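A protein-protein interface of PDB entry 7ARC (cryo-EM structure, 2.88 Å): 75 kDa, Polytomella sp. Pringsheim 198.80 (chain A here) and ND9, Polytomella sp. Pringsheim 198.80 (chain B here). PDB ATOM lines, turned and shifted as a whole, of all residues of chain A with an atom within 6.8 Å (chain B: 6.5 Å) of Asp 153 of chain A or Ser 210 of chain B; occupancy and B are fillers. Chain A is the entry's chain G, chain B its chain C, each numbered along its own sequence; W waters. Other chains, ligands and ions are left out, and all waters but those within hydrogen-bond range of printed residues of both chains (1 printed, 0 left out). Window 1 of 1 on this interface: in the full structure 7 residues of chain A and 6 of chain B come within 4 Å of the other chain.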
ATOM      1  N   MET A 129      31.547   1.156 -24.076  1.00  0.00           N
ATOM      2  CA  MET A 129      30.980   2.485 -23.889  1.00  0.00           C
ATOM      3  C   MET A 129      32.038   3.561 -24.107  1.00  0.00           C
ATOM      4  O   MET A 129      31.770   4.599 -24.730  1.00  0.00           O
ATOM      5  CB  MET A 129      30.392   2.578 -22.483  1.00  0.00           C
ATOM      6  CG  MET A 129      29.497   3.758 -22.235  1.00  0.00           C
ATOM      7  SD  MET A 129      27.985   3.609 -23.189  1.00  0.00           S
ATOM      8  CE  MET A 129      28.148   5.042 -24.229  1.00  0.00           C
ATOM      9  N   GLY A 146      18.479  15.205 -26.244  1.00  0.00           N
ATOM     10  CA  GLY A 146      19.136  15.401 -24.958  1.00  0.00           C
ATOM     11  C   GLY A 146      18.497  14.633 -23.816  1.00  0.00           C
ATOM     12  O   GLY A 146      19.188  13.988 -23.025  1.00  0.00           O
ATOM     13  N   GLY A 147      17.177  14.689 -23.711  1.00  0.00           N
ATOM     14  CA  GLY A 147      16.510  13.979 -22.642  1.00  0.00           C
ATOM     15  C   GLY A 147      16.059  12.581 -22.972  1.00  0.00           C
ATOM     16  O   GLY A 147      15.539  11.879 -22.101  1.00  0.00           O
ATOM     17  N   GLU A 148      16.245  12.152 -24.216  1.00  0.00           N
ATOM     18  CA  GLU A 148      15.718  10.885 -24.705  1.00  0.00           C
ATOM     19  C   GLU A 148      16.796  10.044 -25.375  1.00  0.00           C
ATOM     20  O   GLU A 148      16.483   9.206 -26.224  1.00  0.00           O
ATOM     21  CB  GLU A 148      14.543  11.136 -25.652  1.00  0.00           C
ATOM     22  CG  GLU A 148      14.919  11.853 -26.932  1.00  0.00           C
ATOM     23  CD  GLU A 148      13.718  12.142 -27.808  1.00  0.00           C
ATOM     24  OE1 GLU A 148      12.589  11.799 -27.401  1.00  0.00           O
ATOM     25  OE2 GLU A 148      13.905  12.711 -28.904  1.00  0.00           O
ATOM     26  N   CYS A 149      18.061  10.271 -25.038  1.00  0.00           N
ATOM     27  CA  CYS A 149      19.174   9.604 -25.696  1.00  0.00           C
ATOM     28  C   CYS A 149      19.472   8.269 -25.030  1.00  0.00           C
ATOM     29  O   CYS A 149      19.654   8.203 -23.811  1.00  0.00           O
ATOM     30  CB  CYS A 149      20.421  10.485 -25.671  1.00  0.00           C
ATOM     31  SG  CYS A 149      21.674  10.012 -26.861  1.00  0.00           S
ATOM     32  N   ASP A 150      19.510   7.205 -25.834  1.00  0.00           N
ATOM     33  CA  ASP A 150      19.987   5.921 -25.336  1.00  0.00           C
ATOM     34  C   ASP A 150      21.451   6.007 -24.939  1.00  0.00           C
ATOM     35  O   ASP A 150      21.879   5.374 -23.968  1.00  0.00           O
ATOM     36  CB  ASP A 150      19.780   4.829 -26.386  1.00  0.00           C
ATOM     37  CG  ASP A 150      18.320   4.502 -26.607  1.00  0.00           C
ATOM     38  OD1 ASP A 150      17.524   4.653 -25.658  1.00  0.00           O
ATOM     39  OD2 ASP A 150      17.966   4.081 -27.727  1.00  0.00           O
ATOM     40  N   LEU A 151      22.240   6.766 -25.702  1.00  0.00           N
ATOM     41  CA  LEU A 151      23.674   6.844 -25.454  1.00  0.00           C
ATOM     42  C   LEU A 151      23.953   7.407 -24.066  1.00  0.00           C
ATOM     43  O   LEU A 151      24.747   6.843 -23.307  1.00  0.00           O
ATOM     44  CB  LEU A 151      24.339   7.701 -26.528  1.00  0.00           C
ATOM     45  CG  LEU A 151      25.849   7.595 -26.705  1.00  0.00           C
ATOM     46  CD1 LEU A 151      26.234   6.148 -26.880  1.00  0.00           C
ATOM     47  CD2 LEU A 151      26.302   8.401 -27.891  1.00  0.00           C
ATOM     48  N   GLN A 152      23.286   8.508 -23.705  1.00  0.00           N
ATOM     49  CA  GLN A 152      23.486   9.093 -22.382  1.00  0.00           C
ATOM     50  C   GLN A 152      23.057   8.137 -21.282  1.00  0.00           C
ATOM     51  O   GLN A 152      23.750   7.988 -20.270  1.00  0.00           O
ATOM     52  CB  GLN A 152      22.710  10.400 -22.237  1.00  0.00           C
ATOM     53  CG  GLN A 152      23.169  11.539 -23.097  1.00  0.00           C
ATOM     54  CD  GLN A 152      22.323  12.772 -22.882  1.00  0.00           C
ATOM     55  OE1 GLN A 152      22.842  13.860 -22.649  1.00  0.00           O
ATOM     56  NE2 GLN A 152      21.013  12.604 -22.937  1.00  0.00           N
ATOM     57  N   ASP A 153      21.897   7.504 -21.449  1.00  0.00           N
ATOM     58  CA  ASP A 153      21.356   6.676 -20.382  1.00  0.00           C
ATOM     59  C   ASP A 153      22.225   5.451 -20.145  1.00  0.00           C
ATOM     60  O   ASP A 153      22.505   5.092 -18.996  1.00  0.00           O
ATOM     61  CB  ASP A 153      19.931   6.260 -20.731  1.00  0.00           C
ATOM     62  CG  ASP A 153      18.926   7.360 -20.472  1.00  0.00           C
ATOM     63  OD1 ASP A 153      19.292   8.358 -19.821  1.00  0.00           O
ATOM     64  OD2 ASP A 153      17.768   7.226 -20.919  1.00  0.00           O
ATOM     65  N   GLN A 154      22.687   4.809 -21.220  1.00  0.00           N
ATOM     66  CA  GLN A 154      23.566   3.661 -21.059  1.00  0.00           C
ATOM     67  C   GLN A 154      24.979   4.060 -20.655  1.00  0.00           C
ATOM     68  O   GLN A 154      25.689   3.245 -20.062  1.00  0.00           O
ATOM     69  CB  GLN A 154      23.571   2.838 -22.342  1.00  0.00           C
ATOM     70  CG  GLN A 154      22.250   2.126 -22.576  1.00  0.00           C
ATOM     71  CD  GLN A 154      22.236   1.306 -23.842  1.00  0.00           C
ATOM     72  OE1 GLN A 154      23.023   0.379 -23.999  1.00  0.00           O
ATOM     73  NE2 GLN A 154      21.334   1.639 -24.752  1.00  0.00           N
ATOM     74  N   ALA A 155      25.403   5.290 -20.954  1.00  0.00           N
ATOM     75  CA  ALA A 155      26.652   5.798 -20.403  1.00  0.00           C
ATOM     76  C   ALA A 155      26.554   5.939 -18.891  1.00  0.00           C
ATOM     77  O   ALA A 155      27.475   5.564 -18.158  1.00  0.00           O
ATOM     78  CB  ALA A 155      27.011   7.133 -21.052  1.00  0.00           C
ATOM     79  N   MET A 156      25.445   6.503 -18.411  1.00  0.00           N
ATOM     80  CA  MET A 156      25.239   6.633 -16.973  1.00  0.00           C
ATOM     81  C   MET A 156      25.145   5.270 -16.299  1.00  0.00           C
ATOM     82  O   MET A 156      25.744   5.053 -15.240  1.00  0.00           O
ATOM     83  CB  MET A 156      23.982   7.453 -16.694  1.00  0.00           C
ATOM     84  CG  MET A 156      24.068   8.901 -17.134  1.00  0.00           C
ATOM     85  SD  MET A 156      25.377   9.808 -16.300  1.00  0.00           S
ATOM     86  CE  MET A 156      24.729   9.890 -14.635  1.00  0.00           C
ATOM     87  N   ILE A 157      24.402   4.338 -16.893  1.00  0.00           N
ATOM     88  CA  ILE A 157      24.126   3.070 -16.223  1.00  0.00           C
ATOM     89  C   ILE A 157      25.287   2.095 -16.388  1.00  0.00           C
ATOM     90  O   ILE A 157      25.727   1.468 -15.419  1.00  0.00           O
ATOM     91  CB  ILE A 157      22.806   2.467 -16.733  1.00  0.00           C
ATOM     92  CG1 ILE A 157      21.645   3.428 -16.485  1.00  0.00           C
ATOM     93  CG2 ILE A 157      22.529   1.150 -16.040  1.00  0.00           C
ATOM     94  CD1 ILE A 157      21.417   3.742 -15.029  1.00  0.00           C
ATOM     95  N   PHE A 158      25.806   1.953 -17.607  1.00  0.00           N
ATOM     96  CA  PHE A 158      26.782   0.914 -17.928  1.00  0.00           C
ATOM     97  C   PHE A 158      28.131   1.489 -18.340  1.00  0.00           C
ATOM     98  O   PHE A 158      28.865   0.863 -19.104  1.00  0.00           O
ATOM     99  CB  PHE A 158      26.267  -0.009 -19.033  1.00  0.00           C
ATOM    100  CG  PHE A 158      24.866  -0.490 -18.832  1.00  0.00           C
ATOM    101  CD1 PHE A 158      24.603  -1.556 -17.995  1.00  0.00           C
ATOM    102  CD2 PHE A 158      23.812   0.107 -19.499  1.00  0.00           C
ATOM    103  CE1 PHE A 158      23.316  -2.012 -17.815  1.00  0.00           C
ATOM    104  CE2 PHE A 158      22.522  -0.344 -19.324  1.00  0.00           C
ATOM    105  CZ  PHE A 158      22.274  -1.404 -18.481  1.00  0.00           C
ATOM    106  N   GLY A 159      28.484   2.673 -17.842  1.00  0.00           N
ATOM    107  CA  GLY A 159      29.720   3.309 -18.245  1.00  0.00           C
ATOM    108  C   GLY A 159      30.436   3.930 -17.063  1.00  0.00           C
ATOM    109  O   GLY A 159      29.876   4.089 -15.978  1.00  0.00           O
ATOM    110  N   PHE B 208      11.350  13.144 -15.875  1.00  0.00           N
ATOM    111  CA  PHE B 208      12.754  12.856 -16.123  1.00  0.00           C
ATOM    112  C   PHE B 208      13.081  11.372 -16.115  1.00  0.00           C
ATOM    113  O   PHE B 208      14.246  11.015 -16.314  1.00  0.00           O
ATOM    114  CB  PHE B 208      13.631  13.563 -15.090  1.00  0.00           C
ATOM    115  CG  PHE B 208      13.634  15.052 -15.215  1.00  0.00           C
ATOM    116  CD1 PHE B 208      14.123  15.661 -16.351  1.00  0.00           C
ATOM    117  CD2 PHE B 208      13.181  15.844 -14.179  1.00  0.00           C
ATOM    118  CE1 PHE B 208      14.139  17.030 -16.462  1.00  0.00           C
ATOM    119  CE2 PHE B 208      13.198  17.212 -14.284  1.00  0.00           C
ATOM    120  CZ  PHE B 208      13.676  17.806 -15.429  1.00  0.00           C
ATOM    121  N   SER B 209      12.102  10.502 -15.885  1.00  0.00           N
ATOM    122  CA  SER B 209      12.402   9.083 -15.751  1.00  0.00           C
ATOM    123  C   SER B 209      12.966   8.530 -17.052  1.00  0.00           C
ATOM    124  O   SER B 209      12.495   8.855 -18.144  1.00  0.00           O
ATOM    125  CB  SER B 209      11.145   8.311 -15.357  1.00  0.00           C
ATOM    126  OG  SER B 209      10.114   8.508 -16.307  1.00  0.00           O
ATOM    127  N   SER B 210      13.982   7.683 -16.924  1.00  0.00           N
ATOM    128  CA  SER B 210      14.658   6.956 -17.985  1.00  0.00           C
ATOM    129  C   SER B 210      14.127   5.534 -18.096  1.00  0.00           C
ATOM    130  O   SER B 210      13.850   4.894 -17.080  1.00  0.00           O
ATOM    131  CB  SER B 210      16.162   6.907 -17.725  1.00  0.00           C
ATOM    132  OG  SER B 210      16.823   6.165 -18.730  1.00  0.00           O
ATOM    133  N   PRO B 211      13.953   5.019 -19.312  1.00  0.00           N
ATOM    134  CA  PRO B 211      13.627   3.594 -19.452  1.00  0.00           C
ATOM    135  C   PRO B 211      14.722   2.683 -18.934  1.00  0.00           C
ATOM    136  O   PRO B 211      14.424   1.613 -18.392  1.00  0.00           O
ATOM    137  CB  PRO B 211      13.416   3.431 -20.963  1.00  0.00           C
ATOM    138  CG  PRO B 211      14.142   4.575 -21.574  1.00  0.00           C
ATOM    139  CD  PRO B 211      13.987   5.705 -20.610  1.00  0.00           C
ATOM    140  N   TRP B 212      15.986   3.072 -19.084  1.00  0.00           N
ATOM    141  CA  TRP B 212      17.097   2.190 -18.754  1.00  0.00           C
ATOM    142  C   TRP B 212      17.384   2.097 -17.262  1.00  0.00           C
ATOM    143  O   TRP B 212      18.184   1.243 -16.864  1.00  0.00           O
ATOM    144  CB  TRP B 212      18.355   2.655 -19.488  1.00  0.00           C
ATOM    145  CG  TRP B 212      18.251   2.502 -20.968  1.00  0.00           C
ATOM    146  CD1 TRP B 212      17.943   3.474 -21.871  1.00  0.00           C
ATOM    147  CD2 TRP B 212      18.437   1.300 -21.721  1.00  0.00           C
ATOM    148  NE1 TRP B 212      17.933   2.956 -23.141  1.00  0.00           N
ATOM    149  CE2 TRP B 212      18.233   1.621 -23.075  1.00  0.00           C
ATOM    150  CE3 TRP B 212      18.760  -0.017 -21.381  1.00  0.00           C
ATOM    151  CZ2 TRP B 212      18.342   0.675 -24.091  1.00  0.00           C
ATOM    152  CZ3 TRP B 212      18.870  -0.953 -22.392  1.00  0.00           C
ATOM    153  CH2 TRP B 212      18.659  -0.603 -23.729  1.00  0.00           C
ATOM    154  N   ASP B 213      16.777   2.940 -16.433  1.00  0.00           N
ATOM    155  CA  ASP B 213      17.060   2.893 -15.005  1.00  0.00           C
ATOM    156  C   ASP B 213      16.569   1.582 -14.399  1.00  0.00           C
ATOM    157  O   ASP B 213      15.603   0.974 -14.870  1.00  0.00           O
ATOM    158  CB  ASP B 213      16.462   4.109 -14.280  1.00  0.00           C
ATOM    159  CG  ASP B 213      14.938   4.185 -14.357  1.00  0.00           C
ATOM    160  OD1 ASP B 213      14.424   5.317 -14.477  1.00  0.00           O
ATOM    161  OD2 ASP B 213      14.243   3.153 -14.266  1.00  0.00           O
ATOM    162  N   THR B 214      17.272   1.125 -13.364  1.00  0.00           N
ATOM    163  CA  THR B 214      16.910  -0.104 -12.677  1.00  0.00           C
ATOM    164  C   THR B 214      16.618   0.079 -11.197  1.00  0.00           C
ATOM    165  O   THR B 214      16.010  -0.812 -10.595  1.00  0.00           O
ATOM    166  CB  THR B 214      18.028  -1.149 -12.820  1.00  0.00           C
ATOM    167  OG1 THR B 214      19.230  -0.647 -12.221  1.00  0.00           O
ATOM    168  CG2 THR B 214      18.289  -1.460 -14.282  1.00  0.00           C
HETATM  169  O   HOH W   1      14.998   9.771 -20.271  1.00  0.00           O
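The side-chain hydroxyl (OG) of Ser 210 of chain B sits at hydrogen-bond distance from the side-chain carboxylate (OD2) of Asp 153 of chain A, at 2.6 Å. OD1 of Asp 150 of chain A lies within hydrogen-bond range of NE1 of Trp 212 of chain B.
The side-chain hydroxyl (OG) of Ser 210 of chain B is in hydrogen-bond range of the backbone NH (N) of Trp 212 of chain B (3.2 Å). N of Ser 210 of chain B lies within hydrogen-bond range of OD1 of Asp 213 of chain B (3.4 Å).
Asp 153 of chain A touches Trp 212 of chain B. NE2 of Gln 154 of chain A touches CZ2 of Trp 212 of chain B, at 3.2 Å.
Asp 153 of chain A touches two residues of chain B. Of chain A, only Asp 153 comes within 4 Å of Ser 210 of chain B. Printed residues of chain A within 4 Å of Trp 212 of chain B: Asp 150, Asp 153 and Gln 154. Of the printed residues of chain B, Gln 154 of chain A touches Trp 212. Printed residues of chain B within 4 Å of Asp 150 of chain A: Trp 212 (3.1 Å). Glu 148 of chain A touches none of the printed residues of chain B. The nearest residue of chain A that does not touch Ser 210 of chain B is Ile 157 of chain A (6.0 Å).
Printed residues of chain A that touch a printed residue of chain B: Asp 150, Asp 153 and Gln 154. Hydrophobic or aromatic side chains of chain B within 4 Å of the printed part of chain A: Trp 212. Among the printed residues, 4 pairs touch across the chains.
Water W1 bridges O of Gly 147 of chain A and O of Ser 209 of chain B.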
